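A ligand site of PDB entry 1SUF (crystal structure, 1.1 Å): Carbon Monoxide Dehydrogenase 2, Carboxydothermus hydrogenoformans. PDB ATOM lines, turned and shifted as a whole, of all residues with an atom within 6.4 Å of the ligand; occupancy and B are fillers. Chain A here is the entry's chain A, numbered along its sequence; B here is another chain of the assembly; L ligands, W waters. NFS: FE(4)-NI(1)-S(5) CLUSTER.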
ATOM      1  N   HIS A  93     -22.341 -17.338   3.454  1.00  0.00           N
ATOM      2  CA  HIS A  93     -23.342 -16.337   3.070  1.00  0.00           C
ATOM      3  C   HIS A  93     -24.699 -16.954   3.040  1.00  0.00           C
ATOM      4  O   HIS A  93     -25.694 -16.295   3.359  1.00  0.00           O
ATOM      5  CB  HIS A  93     -22.971 -15.838   1.657  1.00  0.00           C
ATOM      6  CG  HIS A  93     -21.787 -14.941   1.682  1.00  0.00           C
ATOM      7  ND1 HIS A  93     -20.758 -15.049   0.778  1.00  0.00           N
ATOM      8  CD2 HIS A  93     -21.449 -13.909   2.525  1.00  0.00           C
ATOM      9  CE1 HIS A  93     -19.813 -14.111   1.046  1.00  0.00           C
ATOM     10  NE2 HIS A  93     -20.218 -13.434   2.098  1.00  0.00           N
ATOM     11  N   GLY A 260     -18.760  -9.904  13.927  1.00  0.00           N
ATOM     12  CA  GLY A 260     -19.410 -11.010  13.210  1.00  0.00           C
ATOM     13  C   GLY A 260     -20.130 -10.413  12.030  1.00  0.00           C
ATOM     14  O   GLY A 260     -19.551  -9.512  11.371  1.00  0.00           O
ATOM     15  N   HIS A 261     -21.330 -10.945  11.742  1.00  0.00           N
ATOM     16  CA  HIS A 261     -21.955 -10.642  10.451  1.00  0.00           C
ATOM     17  C   HIS A 261     -23.401 -10.291  10.416  1.00  0.00           C
ATOM     18  O   HIS A 261     -23.837  -9.502   9.571  1.00  0.00           O
ATOM     19  CB  HIS A 261     -21.819 -11.950   9.556  1.00  0.00           C
ATOM     20  CG  HIS A 261     -20.443 -11.807   9.002  1.00  0.00           C
ATOM     21  ND1 HIS A 261     -19.312 -12.134   9.754  1.00  0.00           N
ATOM     22  CD2 HIS A 261     -19.989 -11.240   7.862  1.00  0.00           C
ATOM     23  CE1 HIS A 261     -18.227 -11.774   9.052  1.00  0.00           C
ATOM     24  NE2 HIS A 261     -18.633 -11.253   7.910  1.00  0.00           N
ATOM     25  N   CYS A 294     -15.769  -5.534  11.793  1.00  0.00           N
ATOM     26  CA  CYS A 294     -16.116  -6.419  10.679  1.00  0.00           C
ATOM     27  C   CYS A 294     -17.517  -6.107  10.150  1.00  0.00           C
ATOM     28  O   CYS A 294     -18.005  -4.994  10.262  1.00  0.00           O
ATOM     29  CB  CYS A 294     -15.862  -7.850  11.093  1.00  0.00           C
ATOM     30  SG  CYS A 294     -14.114  -8.368  11.057  1.00  0.00           S
ATOM     31  N   CYS A 295     -18.145  -7.101   9.479  1.00  0.00           N
ATOM     32  CA  CYS A 295     -19.322  -6.771   8.692  1.00  0.00           C
ATOM     33  C   CYS A 295     -20.538  -6.416   9.511  1.00  0.00           C
ATOM     34  O   CYS A 295     -21.301  -5.514   9.111  1.00  0.00           O
ATOM     35  CB  CYS A 295     -19.718  -7.983   7.812  1.00  0.00           C
ATOM     36  SG  CYS A 295     -18.830  -8.095   6.230  1.00  0.00           S
ATOM     37  N   THR A 296     -20.744  -7.028  10.665  1.00  0.00           N
ATOM     38  CA  THR A 296     -21.911  -6.591  11.461  1.00  0.00           C
ATOM     39  C   THR A 296     -21.708  -5.149  11.877  1.00  0.00           C
ATOM     40  O   THR A 296     -22.689  -4.360  11.971  1.00  0.00           O
ATOM     41  CB  THR A 296     -22.159  -7.575  12.601  1.00  0.00           C
ATOM     42  OG1 THR A 296     -23.557  -7.430  12.983  1.00  0.00           O
ATOM     43  CG2 THR A 296     -21.344  -7.357  13.839  1.00  0.00           C
ATOM     44  N   HIS A 311     -11.270  -3.496  12.034  1.00  0.00           N
ATOM     45  CA  HIS A 311     -11.679  -4.486  11.047  1.00  0.00           C
ATOM     46  C   HIS A 311     -10.652  -5.618  10.972  1.00  0.00           C
ATOM     47  O   HIS A 311      -9.438  -5.390  11.153  1.00  0.00           O
ATOM     48  CB  HIS A 311     -11.783  -3.887   9.607  1.00  0.00           C
ATOM     49  CG  HIS A 311     -12.705  -2.676   9.596  1.00  0.00           C
ATOM     50  ND1 HIS A 311     -12.249  -1.397   9.921  1.00  0.00           N
ATOM     51  CD2 HIS A 311     -14.033  -2.612   9.345  1.00  0.00           C
ATOM     52  CE1 HIS A 311     -13.328  -0.586   9.832  1.00  0.00           C
ATOM     53  NE2 HIS A 311     -14.411  -1.315   9.478  1.00  0.00           N
ATOM     54  N   SER A 312     -11.146  -6.787  10.607  1.00  0.00           N
ATOM     55  CA  SER A 312     -10.368  -7.891  10.096  1.00  0.00           C
ATOM     56  C   SER A 312      -9.133  -8.162  10.940  1.00  0.00           C
ATOM     57  O   SER A 312      -9.215  -8.463  12.146  1.00  0.00           O
ATOM     58  CB  SER A 312     -10.070  -7.586   8.602  1.00  0.00           C
ATOM     59  OG  SER A 312      -9.581  -8.712   7.885  1.00  0.00           O
ATOM     60  N   VAL A 313      -7.983  -8.097  10.294  1.00  0.00           N
ATOM     61  CA  VAL A 313      -6.759  -8.612  10.929  1.00  0.00           C
ATOM     62  C   VAL A 313      -6.426  -7.919  12.232  1.00  0.00           C
ATOM     63  O   VAL A 313      -5.763  -8.545  13.113  1.00  0.00           O
ATOM     64  CB  VAL A 313      -5.599  -8.493   9.893  1.00  0.00           C
ATOM     65  CG1 VAL A 313      -5.117  -7.046   9.659  1.00  0.00           C
ATOM     66  CG2 VAL A 313      -4.415  -9.323  10.357  1.00  0.00           C
ATOM     67  N   GLN A 315      -8.480  -6.867  14.621  1.00  0.00           N
ATOM     68  CA  GLN A 315      -9.566  -6.898  15.588  1.00  0.00           C
ATOM     69  C   GLN A 315      -9.083  -7.066  17.033  1.00  0.00           C
ATOM     70  O   GLN A 315      -9.739  -6.577  17.976  1.00  0.00           O
ATOM     71  CB  GLN A 315     -10.557  -8.044  15.257  1.00  0.00           C
ATOM     72  CG  GLN A 315      -9.865  -9.418  15.161  1.00  0.00           C
ATOM     73  CD  GLN A 315     -10.880 -10.440  14.664  1.00  0.00           C
ATOM     74  OE1 GLN A 315     -11.542 -11.125  15.458  1.00  0.00           O
ATOM     75  NE2 GLN A 315     -10.992 -10.537  13.347  1.00  0.00           N
ATOM     76  N   GLN A 332     -18.470 -15.890  11.892  1.00  0.00           N
ATOM     77  CA  GLN A 332     -17.569 -15.655  10.798  1.00  0.00           C
ATOM     78  C   GLN A 332     -16.573 -14.523  11.086  1.00  0.00           C
ATOM     79  O   GLN A 332     -16.993 -13.440  11.541  1.00  0.00           O
ATOM     80  CB  GLN A 332     -18.281 -15.368   9.475  1.00  0.00           C
ATOM     81  CG  GLN A 332     -19.292 -16.427   9.014  1.00  0.00           C
ATOM     82  CD  GLN A 332     -20.255 -15.859   7.991  1.00  0.00           C
ATOM     83  OE1 GLN A 332     -20.052 -14.793   7.359  1.00  0.00           O
ATOM     84  NE2 GLN A 332     -21.403 -16.516   7.801  1.00  0.00           N
ATOM     85  N   CYS A 333     -15.293 -14.817  10.775  1.00  0.00           N
ATOM     86  CA  CYS A 333     -14.218 -13.834  10.737  1.00  0.00           C
ATOM     87  C   CYS A 333     -13.788 -13.368  12.116  1.00  0.00           C
ATOM     88  O   CYS A 333     -12.994 -12.398  12.230  1.00  0.00           O
ATOM     89  CB  CYS A 333     -14.613 -12.587   9.878  1.00  0.00           C
ATOM     90  SG  CYS A 333     -14.958 -13.125   8.167  1.00  0.00           S
ATOM     91  N   ALA A 444     -13.177  -4.841  -2.258  1.00  0.00           N
ATOM     92  CA  ALA A 444     -13.966  -5.760  -1.452  1.00  0.00           C
ATOM     93  C   ALA A 444     -13.038  -6.614  -0.627  1.00  0.00           C
ATOM     94  O   ALA A 444     -11.849  -6.704  -0.920  1.00  0.00           O
ATOM     95  CB  ALA A 444     -14.791  -6.668  -2.374  1.00  0.00           C
ATOM     96  N   GLY A 445     -13.622  -7.270   0.368  1.00  0.00           N
ATOM     97  CA  GLY A 445     -12.882  -8.324   1.056  1.00  0.00           C
ATOM     98  C   GLY A 445     -11.969  -7.805   2.143  1.00  0.00           C
ATOM     99  O   GLY A 445     -11.992  -6.634   2.617  1.00  0.00           O
ATOM    100  N   CYS A 446     -11.168  -8.739   2.633  1.00  0.00           N
ATOM    101  CA  CYS A 446     -10.504  -8.740   3.922  1.00  0.00           C
ATOM    102  C   CYS A 446      -9.209  -7.991   3.946  1.00  0.00           C
ATOM    103  O   CYS A 446      -8.741  -7.503   2.900  1.00  0.00           O
ATOM    104  CB  CYS A 446     -10.198 -10.244   4.286  1.00  0.00           C
ATOM    105  SG  CYS A 446     -11.470 -11.420   3.757  1.00  0.00           S
ATOM    106  N   ASN A 447      -8.596  -7.887   5.130  1.00  0.00           N
ATOM    107  CA  ASN A 447      -7.153  -7.772   5.267  1.00  0.00           C
ATOM    108  C   ASN A 447      -6.576  -9.177   5.450  1.00  0.00           C
ATOM    109  O   ASN A 447      -7.299 -10.122   5.764  1.00  0.00           O
ATOM    110  CB  ASN A 447      -6.757  -6.969   6.522  1.00  0.00           C
ATOM    111  CG  ASN A 447      -7.198  -5.504   6.513  1.00  0.00           C
ATOM    112  OD1 ASN A 447      -6.866  -4.740   5.567  1.00  0.00           O
ATOM    113  ND2 ASN A 447      -7.873  -5.114   7.553  1.00  0.00           N
ATOM    114  N   THR A 474     -16.761  -2.162  -0.057  1.00  0.00           N
ATOM    115  CA  THR A 474     -17.589  -2.889   0.923  1.00  0.00           C
ATOM    116  C   THR A 474     -16.672  -3.617   1.904  1.00  0.00           C
ATOM    117  O   THR A 474     -15.456  -3.746   1.707  1.00  0.00           O
ATOM    118  CB  THR A 474     -18.443  -3.976   0.231  1.00  0.00           C
ATOM    119  OG1 THR A 474     -17.498  -4.897  -0.395  1.00  0.00           O
ATOM    120  CG2 THR A 474     -19.350  -3.404  -0.835  1.00  0.00           C
ATOM    121  N   GLY A 475     -17.286  -4.138   2.974  1.00  0.00           N
ATOM    122  CA  GLY A 475     -16.573  -5.016   3.895  1.00  0.00           C
ATOM    123  C   GLY A 475     -15.372  -4.339   4.505  1.00  0.00           C
ATOM    124  O   GLY A 475     -15.345  -3.140   4.828  1.00  0.00           O
ATOM    125  N   CYS A 476     -14.325  -5.143   4.697  1.00  0.00           N
ATOM    126  CA  CYS A 476     -13.127  -4.622   5.334  1.00  0.00           C
ATOM    127  C   CYS A 476     -12.283  -3.853   4.328  1.00  0.00           C
ATOM    128  O   CYS A 476     -11.348  -3.151   4.728  1.00  0.00           O
ATOM    129  CB  CYS A 476     -12.367  -5.741   6.073  1.00  0.00           C
ATOM    130  SG  CYS A 476     -13.402  -6.453   7.435  1.00  0.00           S
ATOM    131  N   GLY A 477     -12.597  -3.903   3.037  1.00  0.00           N
ATOM    132  CA  GLY A 477     -12.011  -2.970   2.079  1.00  0.00           C
ATOM    133  C   GLY A 477     -12.516  -1.547   2.332  1.00  0.00           C
ATOM    134  O   GLY A 477     -11.745  -0.574   2.387  1.00  0.00           O
ATOM    135  N   SER A 525     -21.712  -3.927   3.822  1.00  0.00           N
ATOM    136  CA  SER A 525     -21.045  -5.157   4.258  1.00  0.00           C
ATOM    137  C   SER A 525     -20.690  -6.063   3.092  1.00  0.00           C
ATOM    138  O   SER A 525     -20.923  -5.737   1.913  1.00  0.00           O
ATOM    139  CB  SER A 525     -22.040  -5.901   5.190  1.00  0.00           C
ATOM    140  OG  SER A 525     -23.144  -6.290   4.344  1.00  0.00           O
ATOM    141  N   CYS A 526     -20.094  -7.252   3.385  1.00  0.00           N
ATOM    142  CA  CYS A 526     -19.688  -8.141   2.303  1.00  0.00           C
ATOM    143  C   CYS A 526     -20.897  -8.702   1.565  1.00  0.00           C
ATOM    144  O   CYS A 526     -20.859  -8.831   0.330  1.00  0.00           O
ATOM    145  CB  CYS A 526     -18.850  -9.291   2.881  1.00  0.00           C
ATOM    146  SG  CYS A 526     -17.238  -8.660   3.405  1.00  0.00           S
ATOM    147  N   VAL A 527     -22.007  -9.025   2.243  1.00  0.00           N
ATOM    148  CA  VAL A 527     -23.189  -9.460   1.437  1.00  0.00           C
ATOM    149  C   VAL A 527     -23.647  -8.322   0.541  1.00  0.00           C
ATOM    150  O   VAL A 527     -24.136  -8.547  -0.558  1.00  0.00           O
ATOM    151  CB  VAL A 527     -24.353  -9.973   2.300  1.00  0.00           C
ATOM    152  CG1 VAL A 527     -24.003 -11.307   2.975  1.00  0.00           C
ATOM    153  CG2 VAL A 527     -24.802  -8.989   3.369  1.00  0.00           C
ATOM    154  N   ASN A 529     -21.850  -6.532  -1.236  1.00  0.00           N
ATOM    155  CA  ASN A 529     -21.337  -6.603  -2.614  1.00  0.00           C
ATOM    156  C   ASN A 529     -22.493  -6.796  -3.600  1.00  0.00           C
ATOM    157  O   ASN A 529     -22.408  -6.389  -4.784  1.00  0.00           O
ATOM    158  CB  ASN A 529     -20.311  -7.741  -2.768  1.00  0.00           C
ATOM    159  CG  ASN A 529     -19.003  -7.270  -2.147  1.00  0.00           C
ATOM    160  OD1 ASN A 529     -18.438  -6.244  -2.537  1.00  0.00           O
ATOM    161  ND2 ASN A 529     -18.493  -8.071  -1.171  1.00  0.00           N
ATOM    162  N   MET A 560      -8.741 -12.817   2.380  1.00  0.00           N
ATOM    163  CA  MET A 560      -8.433 -13.848   3.401  1.00  0.00           C
ATOM    164  C   MET A 560      -9.461 -14.996   3.379  1.00  0.00           C
ATOM    165  O   MET A 560      -9.108 -16.185   3.266  1.00  0.00           O
ATOM    166  CB  MET A 560      -8.316 -13.193   4.800  1.00  0.00           C
ATOM    167  CG  MET A 560      -8.057 -14.165   5.930  1.00  0.00           C
ATOM    168  SD  MET A 560      -9.530 -14.815   6.769  1.00  0.00           S
ATOM    169  CE  MET A 560     -10.308 -13.266   7.347  1.00  0.00           C
ATOM    170  N   HIS A 561     -10.734 -14.672   3.564  1.00  0.00           N
ATOM    171  CA  HIS A 561     -11.709 -15.722   3.912  1.00  0.00           C
ATOM    172  C   HIS A 561     -12.129 -16.531   2.690  1.00  0.00           C
ATOM    173  O   HIS A 561     -12.085 -16.038   1.558  1.00  0.00           O
ATOM    174  CB  HIS A 561     -12.908 -15.034   4.599  1.00  0.00           C
ATOM    175  CG  HIS A 561     -13.768 -15.969   5.403  1.00  0.00           C
ATOM    176  ND1 HIS A 561     -14.695 -16.826   4.846  1.00  0.00           N
ATOM    177  CD2 HIS A 561     -13.759 -16.164   6.749  1.00  0.00           C
ATOM    178  CE1 HIS A 561     -15.260 -17.520   5.836  1.00  0.00           C
ATOM    179  NE2 HIS A 561     -14.719 -17.128   7.014  1.00  0.00           N
ATOM    180  N   LYS A 563     -15.107 -16.892   2.005  1.00  0.00           N
ATOM    181  CA  LYS A 563     -16.133 -16.000   1.432  1.00  0.00           C
ATOM    182  C   LYS A 563     -15.585 -15.057   0.377  1.00  0.00           C
ATOM    183  O   LYS A 563     -16.287 -14.739  -0.595  1.00  0.00           O
ATOM    184  CB  LYS A 563     -16.802 -15.187   2.560  1.00  0.00           C
ATOM    185  CG  LYS A 563     -17.764 -16.039   3.416  1.00  0.00           C
ATOM    186  CD  LYS A 563     -18.353 -15.202   4.568  1.00  0.00           C
ATOM    187  CE  LYS A 563     -17.270 -14.821   5.589  1.00  0.00           C
ATOM    188  NZ  LYS A 563     -17.711 -13.650   6.433  1.00  0.00           N
ATOM    189  N   ALA A 564     -14.357 -14.540   0.583  1.00  0.00           N
ATOM    190  CA  ALA A 564     -13.779 -13.635  -0.404  1.00  0.00           C
ATOM    191  C   ALA A 564     -13.413 -14.392  -1.675  1.00  0.00           C
ATOM    192  O   ALA A 564     -13.489 -13.828  -2.770  1.00  0.00           O
ATOM    193  CB  ALA A 564     -12.548 -12.953   0.216  1.00  0.00           C
ATOM    194  N   ILE A 567     -16.754 -14.688  -3.513  1.00  0.00           N
ATOM    195  CA  ILE A 567     -17.148 -13.381  -4.095  1.00  0.00           C
ATOM    196  C   ILE A 567     -16.278 -13.072  -5.307  1.00  0.00           C
ATOM    197  O   ILE A 567     -16.774 -12.660  -6.346  1.00  0.00           O
ATOM    198  CB  ILE A 567     -17.076 -12.287  -3.019  1.00  0.00           C
ATOM    199  CG1 ILE A 567     -18.248 -12.383  -2.034  1.00  0.00           C
ATOM    200  CG2 ILE A 567     -17.037 -10.899  -3.712  1.00  0.00           C
ATOM    201  CD1 ILE A 567     -18.019 -11.677  -0.707  1.00  0.00           C
ATOM    202  N   MET B 199     -13.366 -20.042   8.434  1.00  0.00           N
ATOM    203  CA  MET B 199     -12.561 -19.275   9.367  1.00  0.00           C
ATOM    204  C   MET B 199     -13.438 -18.396  10.250  1.00  0.00           C
ATOM    205  O   MET B 199     -14.393 -17.729   9.805  1.00  0.00           O
ATOM    206  CB  MET B 199     -11.515 -18.450   8.557  1.00  0.00           C
ATOM    207  CG  MET B 199     -10.613 -17.610   9.480  1.00  0.00           C
ATOM    208  SD  MET B 199     -11.345 -15.997   9.872  1.00  0.00           S
ATOM    209  CE  MET B 199     -10.592 -15.610  11.459  1.00  0.00           C
HETATM  210 NI1  NFS L   1     -15.787 -10.185   3.797  1.00  0.00          NI
HETATM  211 FE1  NFS L   1     -17.543 -10.004   6.359  1.00  0.00          FE
HETATM  212 FE2  NFS L   1     -13.938  -8.600   6.740  1.00  0.00          FE
HETATM  213 FE3  NFS L   1     -13.287 -10.538   4.991  1.00  0.00          FE
HETATM  214 FE4  NFS L   1     -14.622 -11.162   7.064  1.00  0.00          FE
HETATM  215  S1  NFS L   1     -15.846  -9.375   7.775  1.00  0.00           S
HETATM  216  S3  NFS L   1     -15.089 -11.928   4.897  1.00  0.00           S
HETATM  217  S4  NFS L   1     -12.435 -10.314   7.194  1.00  0.00           S
HETATM  218  S5  NFS L   1     -14.174  -8.472   4.462  1.00  0.00           S
HETATM  219  O   HOH W   1     -15.207 -11.265   1.240  1.00  0.00           O
HETATM  220  O   HOH W   2     -11.333 -11.292  10.304  1.00  0.00           O
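Water W1 bridges N of Ala 564 and S3 of the ligand. Water W2 lies within hydrogen-bond range of O of Cys 333 (2.8 Å), NE2 of Gln 315 (3.2 Å) and S4 of the ligand (3.4 Å).
S5 of the ligand lies close to O of Gly 445. Merely in contact with the ligand: Cys 294, Met 560 and His 561. Of the 30 residues printed, 12 come within 4 Å of the ligand. The nearest printed residue that does not touch the ligand is Gly 475 (4.2 Å).
S4 of the ligand lies close to OG of Ser 312. NZ of Lys 563 sits close to S3 of the ligand (3.5 Å). An iron atom (FE3) of the ligand is bound by the side-chain sulfur (SG) of Cys 446, 2.4 Å away. The backbone NH (N) of Cys 446 sits close to a sulfur (S5) of the ligand, at 3.5 Å. SG of Cys 526 is bound to NI1 of the ligand, at 2.1 Å. The side-chain sulfur (SG) of Cys 476 binds an iron atom (FE2) of the ligand (2.3 Å). The side-chain sulfur (SG) of Cys 333 binds an iron atom (FE4) of the ligand (2.3 Å). The backbone NH of Cys 476 sits close to a sulfur (S5) of the ligand (3.3 Å). An iron atom (FE1) of the ligand is bound by a ring nitrogen (NE2) of His 261 (2.3 Å). The backbone NH of Cys 295 sits close to a sulfur (S1) of the ligand, 3.7 Å away. FE1 of the ligand is bound by SG of Cys 295 (2.3 Å).
The backbone carbonyl oxygen (O) of Ser 312 sits at hydrogen-bond distance from the side-chain amide nitrogen (NE2) of Gln 315 (3.0 Å). N of His 561 lies close to SG of Cys 446 (3.3 Å). N of Lys 563 lies within hydrogen-bond range of ND1 of His 561. The backbone carbonyl oxygen (O) of Cys 333 lies within hydrogen-bond range of the side-chain amide nitrogen (NE2) of Gln 315, 3.0 Å away. N of Asn 447 lies within hydrogen-bond range of OG of Ser 312 (3.0 Å). ND1 of His 261 is in hydrogen-bond range of O of Gln 332 (3.2 Å). The backbone carbonyl oxygen of Gly 445 lies close to the backbone NH of Cys 476. SG of Cys 446 sits close to N of Met 560 (3.4 Å).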
